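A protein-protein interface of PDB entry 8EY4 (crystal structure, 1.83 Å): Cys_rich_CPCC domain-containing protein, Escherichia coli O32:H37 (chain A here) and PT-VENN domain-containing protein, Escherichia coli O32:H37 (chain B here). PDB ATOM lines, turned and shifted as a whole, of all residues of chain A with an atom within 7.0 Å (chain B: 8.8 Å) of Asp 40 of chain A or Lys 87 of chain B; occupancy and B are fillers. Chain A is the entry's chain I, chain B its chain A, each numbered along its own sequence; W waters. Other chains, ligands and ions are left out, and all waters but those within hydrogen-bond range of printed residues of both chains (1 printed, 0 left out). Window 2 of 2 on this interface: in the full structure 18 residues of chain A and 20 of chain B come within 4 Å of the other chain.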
ATOM      1  N   ASP A  34     -33.993  10.400  33.245  1.00  0.00           N
ATOM      2  CA  ASP A  34     -33.098   9.513  32.500  1.00  0.00           C
ATOM      3  C   ASP A  34     -31.645   9.886  32.776  1.00  0.00           C
ATOM      4  O   ASP A  34     -31.245  11.022  32.481  1.00  0.00           O
ATOM      5  CB  ASP A  34     -33.417   9.670  31.024  1.00  0.00           C
ATOM      6  CG  ASP A  34     -32.518   8.837  30.091  1.00  0.00           C
ATOM      7  OD1 ASP A  34     -31.311   8.710  30.327  1.00  0.00           O
ATOM      8  OD2 ASP A  34     -33.031   8.359  29.067  1.00  0.00           O
ATOM      9  N   PRO A  35     -30.815   8.973  33.289  1.00  0.00           N
ATOM     10  CA  PRO A  35     -29.467   9.377  33.711  1.00  0.00           C
ATOM     11  C   PRO A  35     -28.527   9.635  32.536  1.00  0.00           C
ATOM     12  O   PRO A  35     -27.574  10.413  32.677  1.00  0.00           O
ATOM     13  CB  PRO A  35     -29.002   8.190  34.572  1.00  0.00           C
ATOM     14  CG  PRO A  35     -29.723   7.009  33.962  1.00  0.00           C
ATOM     15  CD  PRO A  35     -31.066   7.534  33.512  1.00  0.00           C
ATOM     16  N   VAL A  36     -28.770   9.016  31.378  1.00  0.00           N
ATOM     17  CA  VAL A  36     -27.975   9.348  30.191  1.00  0.00           C
ATOM     18  C   VAL A  36     -28.196  10.806  29.801  1.00  0.00           C
ATOM     19  O   VAL A  36     -27.250  11.520  29.437  1.00  0.00           O
ATOM     20  CB  VAL A  36     -28.338   8.393  29.043  1.00  0.00           C
ATOM     21  CG1 VAL A  36     -27.670   8.811  27.732  1.00  0.00           C
ATOM     22  CG2 VAL A  36     -27.907   7.000  29.422  1.00  0.00           C
ATOM     23  N   GLN A  37     -29.447  11.268  29.879  1.00  0.00           N
ATOM     24  CA  GLN A  37     -29.784  12.620  29.445  1.00  0.00           C
ATOM     25  C   GLN A  37     -29.420  13.683  30.479  1.00  0.00           C
ATOM     26  O   GLN A  37     -29.193  14.835  30.094  1.00  0.00           O
ATOM     27  CB  GLN A  37     -31.269  12.699  29.085  1.00  0.00           C
ATOM     28  CG  GLN A  37     -31.563  11.917  27.796  1.00  0.00           C
ATOM     29  CD  GLN A  37     -32.991  12.082  27.303  1.00  0.00           C
ATOM     30  OE1 GLN A  37     -33.912  11.551  27.908  1.00  0.00           O
ATOM     31  NE2 GLN A  37     -33.177  12.789  26.182  1.00  0.00           N
ATOM     32  N   SER A  38     -29.377  13.347  31.783  1.00  0.00           N
ATOM     33  CA  SER A  38     -28.795  14.311  32.721  1.00  0.00           C
ATOM     34  C   SER A  38     -27.269  14.323  32.648  1.00  0.00           C
ATOM     35  O   SER A  38     -26.650  15.381  32.832  1.00  0.00           O
ATOM     36  CB  SER A  38     -29.292  14.060  34.160  1.00  0.00           C
ATOM     37  OG  SER A  38     -28.885  12.806  34.684  1.00  0.00           O
ATOM     38  N   ALA A  39     -26.629  13.192  32.353  1.00  0.00           N
ATOM     39  CA  ALA A  39     -25.171  13.219  32.211  1.00  0.00           C
ATOM     40  C   ALA A  39     -24.742  13.942  30.935  1.00  0.00           C
ATOM     41  O   ALA A  39     -23.642  14.500  30.880  1.00  0.00           O
ATOM     42  CB  ALA A  39     -24.605  11.798  32.236  1.00  0.00           C
ATOM     43  N   ASP A  40     -25.589  13.948  29.908  1.00  0.00           N
ATOM     44  CA  ASP A  40     -25.334  14.661  28.658  1.00  0.00           C
ATOM     45  C   ASP A  40     -26.564  15.494  28.330  1.00  0.00           C
ATOM     46  O   ASP A  40     -27.498  15.023  27.658  1.00  0.00           O
ATOM     47  CB  ASP A  40     -25.032  13.682  27.534  1.00  0.00           C
ATOM     48  CG  ASP A  40     -24.685  14.384  26.235  1.00  0.00           C
ATOM     49  OD1 ASP A  40     -24.816  15.635  26.155  1.00  0.00           O
ATOM     50  OD2 ASP A  40     -24.295  13.667  25.301  1.00  0.00           O
ATOM     51  N   PRO A  41     -26.614  16.741  28.801  1.00  0.00           N
ATOM     52  CA  PRO A  41     -27.869  17.497  28.694  1.00  0.00           C
ATOM     53  C   PRO A  41     -28.229  17.905  27.278  1.00  0.00           C
ATOM     54  O   PRO A  41     -29.320  18.453  27.084  1.00  0.00           O
ATOM     55  CB  PRO A  41     -27.626  18.727  29.588  1.00  0.00           C
ATOM     56  CG  PRO A  41     -26.540  18.297  30.510  1.00  0.00           C
ATOM     57  CD  PRO A  41     -25.647  17.398  29.685  1.00  0.00           C
ATOM     58  N   ASP A  42     -27.353  17.692  26.297  1.00  0.00           N
ATOM     59  CA  ASP A  42     -27.676  17.980  24.909  1.00  0.00           C
ATOM     60  C   ASP A  42     -28.111  16.744  24.131  1.00  0.00           C
ATOM     61  O   ASP A  42     -28.392  16.852  22.933  1.00  0.00           O
ATOM     62  CB  ASP A  42     -26.489  18.633  24.212  1.00  0.00           C
ATOM     63  CG  ASP A  42     -26.364  20.108  24.556  1.00  0.00           C
ATOM     64  OD1 ASP A  42     -27.410  20.765  24.795  1.00  0.00           O
ATOM     65  OD2 ASP A  42     -25.224  20.602  24.586  1.00  0.00           O
ATOM     66  N   PHE A  43     -28.247  15.597  24.788  1.00  0.00           N
ATOM     67  CA  PHE A  43     -28.546  14.339  24.095  1.00  0.00           C
ATOM     68  C   PHE A  43     -30.061  14.172  24.023  1.00  0.00           C
ATOM     69  O   PHE A  43     -30.716  13.949  25.050  1.00  0.00           O
ATOM     70  CB  PHE A  43     -27.893  13.171  24.827  1.00  0.00           C
ATOM     71  CG  PHE A  43     -28.082  11.824  24.137  1.00  0.00           C
ATOM     72  CD1 PHE A  43     -27.179  11.385  23.180  1.00  0.00           C
ATOM     73  CD2 PHE A  43     -29.155  11.000  24.465  1.00  0.00           C
ATOM     74  CE1 PHE A  43     -27.341  10.131  22.549  1.00  0.00           C
ATOM     75  CE2 PHE A  43     -29.313   9.746  23.829  1.00  0.00           C
ATOM     76  CZ  PHE A  43     -28.407   9.325  22.893  1.00  0.00           C
ATOM     77  N   SER A  44     -30.622  14.324  22.822  1.00  0.00           N
ATOM     78  CA  SER A  44     -32.042  14.084  22.630  1.00  0.00           C
ATOM     79  C   SER A  44     -32.285  12.595  22.403  1.00  0.00           C
ATOM     80  O   SER A  44     -31.377  11.838  22.049  1.00  0.00           O
ATOM     81  CB  SER A  44     -32.586  14.869  21.438  1.00  0.00           C
ATOM     82  OG  SER A  44     -32.049  14.371  20.211  1.00  0.00           O
ATOM     83  N   SER A  51     -33.716  16.844  24.313  1.00  0.00           N
ATOM     84  CA  SER A  51     -32.625  16.883  25.267  1.00  0.00           C
ATOM     85  C   SER A  51     -33.079  17.582  26.551  1.00  0.00           C
ATOM     86  O   SER A  51     -34.106  18.276  26.585  1.00  0.00           O
ATOM     87  CB  SER A  51     -31.421  17.623  24.690  1.00  0.00           C
ATOM     88  OG  SER A  51     -31.690  19.016  24.540  1.00  0.00           O
ATOM     89  N   LEU A  52     -32.288  17.399  27.615  1.00  0.00           N
ATOM     90  CA  LEU A  52     -32.571  18.097  28.873  1.00  0.00           C
ATOM     91  C   LEU A  52     -32.542  19.606  28.682  1.00  0.00           C
ATOM     92  O   LEU A  52     -33.387  20.328  29.236  1.00  0.00           O
ATOM     93  CB  LEU A  52     -31.578  17.683  29.964  1.00  0.00           C
ATOM     94  CG  LEU A  52     -31.729  18.336  31.357  1.00  0.00           C
ATOM     95  CD1 LEU A  52     -33.164  18.314  31.882  1.00  0.00           C
ATOM     96  CD2 LEU A  52     -30.779  17.665  32.372  1.00  0.00           C
ATOM     97  N   ASN A  53     -31.570  20.101  27.911  1.00  0.00           N
ATOM     98  CA  ASN A  53     -31.467  21.545  27.697  1.00  0.00           C
ATOM     99  C   ASN A  53     -32.661  22.082  26.925  1.00  0.00           C
ATOM    100  O   ASN A  53     -33.120  23.207  27.181  1.00  0.00           O
ATOM    101  CB  ASN A  53     -30.158  21.876  26.978  1.00  0.00           C
ATOM    102  CG  ASN A  53     -28.980  21.907  27.930  1.00  0.00           C
ATOM    103  OD1 ASN A  53     -29.157  22.107  29.129  1.00  0.00           O
ATOM    104  ND2 ASN A  53     -27.773  21.724  27.403  1.00  0.00           N
ATOM    105  N   LYS B  46     -27.215  -4.665  31.248  1.00  0.00           N
ATOM    106  CA  LYS B  46     -26.225  -3.973  32.052  1.00  0.00           C
ATOM    107  C   LYS B  46     -26.780  -3.856  33.468  1.00  0.00           C
ATOM    108  O   LYS B  46     -27.994  -3.866  33.664  1.00  0.00           O
ATOM    109  CB  LYS B  46     -25.911  -2.591  31.458  1.00  0.00           C
ATOM    110  CG  LYS B  46     -25.016  -2.629  30.210  1.00  0.00           C
ATOM    111  CD  LYS B  46     -25.094  -1.340  29.385  1.00  0.00           C
ATOM    112  CE  LYS B  46     -24.099  -1.355  28.231  1.00  0.00           C
ATOM    113  NZ  LYS B  46     -24.318  -0.262  27.256  1.00  0.00           N
ATOM    114  N   ARG B  48     -26.756  -1.515  37.088  1.00  0.00           N
ATOM    115  CA  ARG B  48     -26.346  -0.211  37.570  1.00  0.00           C
ATOM    116  C   ARG B  48     -25.872  -0.294  39.017  1.00  0.00           C
ATOM    117  O   ARG B  48     -26.037  -1.327  39.681  1.00  0.00           O
ATOM    118  CB  ARG B  48     -27.501   0.790  37.401  1.00  0.00           C
ATOM    119  CG  ARG B  48     -27.448   1.363  35.959  1.00  0.00           C
ATOM    120  CD  ARG B  48     -28.271   2.614  35.683  1.00  0.00           C
ATOM    121  NE  ARG B  48     -28.153   3.709  36.646  1.00  0.00           N
ATOM    122  CZ  ARG B  48     -27.456   4.836  36.446  1.00  0.00           C
ATOM    123  NH1 ARG B  48     -26.770   5.020  35.329  1.00  0.00           N
ATOM    124  NH2 ARG B  48     -27.452   5.790  37.376  1.00  0.00           N
ATOM    125  N   LEU B  54     -30.665  -3.073  33.455  1.00  0.00           N
ATOM    126  CA  LEU B  54     -31.134  -2.466  32.218  1.00  0.00           C
ATOM    127  C   LEU B  54     -31.186  -3.499  31.105  1.00  0.00           C
ATOM    128  O   LEU B  54     -30.311  -4.373  31.019  1.00  0.00           O
ATOM    129  CB  LEU B  54     -30.201  -1.345  31.760  1.00  0.00           C
ATOM    130  CG  LEU B  54     -29.677  -0.438  32.851  1.00  0.00           C
ATOM    131  CD1 LEU B  54     -28.699   0.562  32.216  1.00  0.00           C
ATOM    132  CD2 LEU B  54     -30.851   0.302  33.441  1.00  0.00           C
ATOM    133  N   LYS B  80     -32.862   7.378  19.653  1.00  0.00           N
ATOM    134  CA  LYS B  80     -31.449   7.172  19.309  1.00  0.00           C
ATOM    135  C   LYS B  80     -31.059   5.697  19.198  1.00  0.00           C
ATOM    136  O   LYS B  80     -29.963   5.387  18.694  1.00  0.00           O
ATOM    137  CB  LYS B  80     -30.567   7.873  20.346  1.00  0.00           C
ATOM    138  CG  LYS B  80     -30.626   9.393  20.240  1.00  0.00           C
ATOM    139  CD  LYS B  80     -29.796   9.901  19.061  1.00  0.00           C
ATOM    140  CE  LYS B  80     -29.878  11.422  18.917  1.00  0.00           C
ATOM    141  NZ  LYS B  80     -29.433  12.049  20.160  1.00  0.00           N
ATOM    142  N   GLY B  81     -31.914   4.777  19.634  1.00  0.00           N
ATOM    143  CA  GLY B  81     -31.628   3.372  19.331  1.00  0.00           C
ATOM    144  C   GLY B  81     -30.370   2.920  20.040  1.00  0.00           C
ATOM    145  O   GLY B  81     -30.135   3.258  21.200  1.00  0.00           O
ATOM    146  N   ILE B  82     -29.522   2.164  19.328  1.00  0.00           N
ATOM    147  CA  ILE B  82     -28.347   1.577  19.973  1.00  0.00           C
ATOM    148  C   ILE B  82     -27.406   2.649  20.503  1.00  0.00           C
ATOM    149  O   ILE B  82     -26.634   2.409  21.441  1.00  0.00           O
ATOM    150  CB  ILE B  82     -27.622   0.634  18.991  1.00  0.00           C
ATOM    151  CG1 ILE B  82     -26.534  -0.152  19.713  1.00  0.00           C
ATOM    152  CG2 ILE B  82     -27.026   1.418  17.824  1.00  0.00           C
ATOM    153  CD1 ILE B  82     -27.053  -1.175  20.623  1.00  0.00           C
ATOM    154  N   GLU B  83     -27.423   3.839  19.905  1.00  0.00           N
ATOM    155  CA  GLU B  83     -26.556   4.896  20.400  1.00  0.00           C
ATOM    156  C   GLU B  83     -26.894   5.245  21.849  1.00  0.00           C
ATOM    157  O   GLU B  83     -26.001   5.566  22.651  1.00  0.00           O
ATOM    158  CB  GLU B  83     -26.682   6.125  19.509  1.00  0.00           C
ATOM    159  CG  GLU B  83     -25.895   7.304  20.023  1.00  0.00           C
ATOM    160  CD  GLU B  83     -25.943   8.463  19.060  1.00  0.00           C
ATOM    161  OE1 GLU B  83     -26.485   8.275  17.946  1.00  0.00           O
ATOM    162  OE2 GLU B  83     -25.442   9.551  19.407  1.00  0.00           O
ATOM    163  N   TYR B  84     -28.181   5.219  22.186  1.00  0.00           N
ATOM    164  CA  TYR B  84     -28.615   5.387  23.572  1.00  0.00           C
ATOM    165  C   TYR B  84     -28.043   4.288  24.463  1.00  0.00           C
ATOM    166  O   TYR B  84     -27.533   4.553  25.551  1.00  0.00           O
ATOM    167  CB  TYR B  84     -30.138   5.372  23.621  1.00  0.00           C
ATOM    168  CG  TYR B  84     -30.700   5.512  25.026  1.00  0.00           C
ATOM    169  CD1 TYR B  84     -30.595   6.716  25.707  1.00  0.00           C
ATOM    170  CD2 TYR B  84     -31.278   4.422  25.676  1.00  0.00           C
ATOM    171  CE1 TYR B  84     -31.081   6.845  26.999  1.00  0.00           C
ATOM    172  CE2 TYR B  84     -31.785   4.543  26.980  1.00  0.00           C
ATOM    173  CZ  TYR B  84     -31.673   5.761  27.633  1.00  0.00           C
ATOM    174  OH  TYR B  84     -32.163   5.916  28.910  1.00  0.00           O
ATOM    175  N   TRP B  85     -28.113   3.032  24.007  1.00  0.00           N
ATOM    176  CA  TRP B  85     -27.570   1.935  24.808  1.00  0.00           C
ATOM    177  C   TRP B  85     -26.086   2.112  25.051  1.00  0.00           C
ATOM    178  O   TRP B  85     -25.595   1.894  26.165  1.00  0.00           O
ATOM    179  CB  TRP B  85     -27.808   0.595  24.097  1.00  0.00           C
ATOM    180  CG  TRP B  85     -27.314  -0.638  24.852  1.00  0.00           C
ATOM    181  CD1 TRP B  85     -26.331  -1.524  24.454  1.00  0.00           C
ATOM    182  CD2 TRP B  85     -27.826  -1.149  26.094  1.00  0.00           C
ATOM    183  NE1 TRP B  85     -26.186  -2.524  25.388  1.00  0.00           N
ATOM    184  CE2 TRP B  85     -27.101  -2.325  26.398  1.00  0.00           C
ATOM    185  CE3 TRP B  85     -28.813  -0.708  26.998  1.00  0.00           C
ATOM    186  CZ2 TRP B  85     -27.354  -3.086  27.551  1.00  0.00           C
ATOM    187  CZ3 TRP B  85     -29.058  -1.461  28.149  1.00  0.00           C
ATOM    188  CH2 TRP B  85     -28.336  -2.636  28.416  1.00  0.00           C
ATOM    189  N   ASN B  86     -25.333   2.432  23.993  1.00  0.00           N
ATOM    190  CA  ASN B  86     -23.888   2.519  24.125  1.00  0.00           C
ATOM    191  C   ASN B  86     -23.435   3.740  24.920  1.00  0.00           C
ATOM    192  O   ASN B  86     -22.242   3.845  25.225  1.00  0.00           O
ATOM    193  CB  ASN B  86     -23.246   2.484  22.733  1.00  0.00           C
ATOM    194  CG  ASN B  86     -23.414   1.124  22.061  1.00  0.00           C
ATOM    195  OD1 ASN B  86     -23.480   0.097  22.737  1.00  0.00           O
ATOM    196  ND2 ASN B  86     -23.485   1.112  20.736  1.00  0.00           N
ATOM    197  N   LYS B  87     -24.355   4.622  25.304  1.00  0.00           N
ATOM    198  CA  LYS B  87     -24.009   5.757  26.146  1.00  0.00           C
ATOM    199  C   LYS B  87     -24.006   5.414  27.623  1.00  0.00           C
ATOM    200  O   LYS B  87     -23.506   6.205  28.429  1.00  0.00           O
ATOM    201  CB  LYS B  87     -24.958   6.936  25.897  1.00  0.00           C
ATOM    202  CG  LYS B  87     -24.480   7.857  24.782  1.00  0.00           C
ATOM    203  CD  LYS B  87     -25.070   9.239  24.916  1.00  0.00           C
ATOM    204  CE  LYS B  87     -24.205  10.186  25.753  1.00  0.00           C
ATOM    205  NZ  LYS B  87     -23.054  10.743  24.996  1.00  0.00           N
ATOM    206  N   GLN B  88     -24.507   4.257  28.016  1.00  0.00           N
ATOM    207  CA  GLN B  88     -24.381   3.927  29.426  1.00  0.00           C
ATOM    208  C   GLN B  88     -23.553   2.677  29.651  1.00  0.00           C
ATOM    209  O   GLN B  88     -23.040   2.078  28.702  1.00  0.00           O
ATOM    210  CB  GLN B  88     -25.742   3.747  30.046  1.00  0.00           C
ATOM    211  CG  GLN B  88     -26.609   2.845  29.230  1.00  0.00           C
ATOM    212  CD  GLN B  88     -28.033   3.293  29.324  1.00  0.00           C
ATOM    213  OE1 GLN B  88     -28.519   3.590  30.409  1.00  0.00           O
ATOM    214  NE2 GLN B  88     -28.704   3.399  28.177  1.00  0.00           N
ATOM    215  OXT GLN B  88     -23.404   2.265  30.804  1.00  0.00           O
HETATM  216  O   HOH W   1     -28.858  14.740  20.259  1.00  0.00           O
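Water W1 lies within hydrogen-bond range of the side-chain amino group (NZ) of Lys 80 of chain B, the backbone NH (N) of Ser 44 of chain A and the backbone carbonyl oxygen (O) of Asp 42 of chain A.
The side-chain hydroxyl (OG) of Ser 38 of chain A is in hydrogen-bond range of the backbone carbonyl oxygen (O) of Pro 35 of chain A, at 3.4 Å. The side-chain carboxylate (OD1) of Asp 40 of chain A sits close to the backbone NH (N) of Asp 42 of chain A, at 3.3 Å. The side-chain carboxylate (OD1) of Asp 34 of chain A lies within hydrogen-bond range of the backbone NH (N) of Gln 37 of chain A, 3.2 Å away. NE2 of Gln 37 of chain A lies within hydrogen-bond range of O of Phe 43 of chain A. The backbone carbonyl oxygen (O) of Tyr 84 of chain B sits at hydrogen-bond distance from the side-chain amide nitrogen (NE2) of Gln 88 of chain B (3.1 Å). The side-chain amino group (NZ) of Lys 46 of chain B lies within salt-bridge range of the chain-end carboxylate (O) of Gln 88 of chain B (3.0 Å).
Hydrophobic or aromatic side chains of chain B that line the printed part of chain A: Tyr 84. Along chain B the printed residues that touch a printed residue of chain A span positions 48 to 88. Of the 14 printed residues of chain A, 6 touch a printed residue of chain B. Printed residues of chain A that touch a printed residue of chain B: Asp 34, Pro 35, Val 36, Asp 40, Phe 43 and Ser 44. Hydrophobic or aromatic side chains of chain A that line the printed part of chain B: Pro 35, Val 36 and Phe 43. Among the printed residues, 11 pairs touch across the chains. Among the printed residues, Asp or Glu carboxylates within 4 Å of a Lys or Arg side-chain nitrogen of the other chain: Asp 40 of chain A with Lys 87 of chain B (3.2 Å).
Of the printed residues of chain B, Pro 35 of chain A touches Arg 48 (3.8 Å). No residue of chain B comes within 4 Å of Ala 39 of chain A. Asp 40 of chain A touches one residue of chain B. No residue of chain B comes within 4 Å of Pro 41 of chain A. Asn 53 of chain A touches none of the printed residues of chain B. Of the printed residues of chain A, Lys 80 of chain B touches Phe 43 (3.5 Å) and Ser 44 (2.7 Å). Gly 81 of chain B touches none of the printed residues of chain A. Printed residues of chain A within 4 Å of Tyr 84 of chain B: Asp 34 (2.6 Å), Val 36 (3.8 Å) and Phe 43 (3.8 Å). Of chain A, only Val 36 (3.8 Å), Asp 40 (3.2 Å) and Phe 43 (3.4 Å) come within 4 Å of Lys 87 of chain B. The nearest residue of chain A that does not touch Lys 87 of chain B is Ala 39 of chain A (6.4 Å). The nearest printed residue of chain A that does not touch Gln 88 of chain B is Pro 35 of chain A (5.1 Å).
OH of Tyr 84 of chain B sits at hydrogen-bond distance from OD2 of Asp 34 of chain A (2.6 Å). OD2 of Asp 40 of chain A is in salt-bridge range of NZ of Lys 87 of chain B, 3.2 Å away. The side-chain amino group (NZ) of Lys 80 of chain B is in hydrogen-bond range of the backbone carbonyl oxygen (O) of Ser 44 of chain A (2.7 Å).
CG of Pro 35 of chain A touches NH1 of Arg 48 of chain B, 3.8 Å away. CB of Val 36 of chain A touches CE1 of Tyr 84 of chain B (3.8 Å). Val 36 of chain A touches Lys 87 of chain B. CG2 of Val 36 of chain A touches OE1 of Gln 88 of chain B (3.6 Å). Phe 43 of chain A touches Lys 80 of chain B. Glu 83 of chain B touches Phe 43 of chain A (OE2 to CE1, 3.7 Å). CE2 of Phe 43 of chain A touches CD1 of Tyr 84 of chain B (3.8 Å). Lys 87 of chain B touches Phe 43 of chain A (CD to CE1, 3.4 Å).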
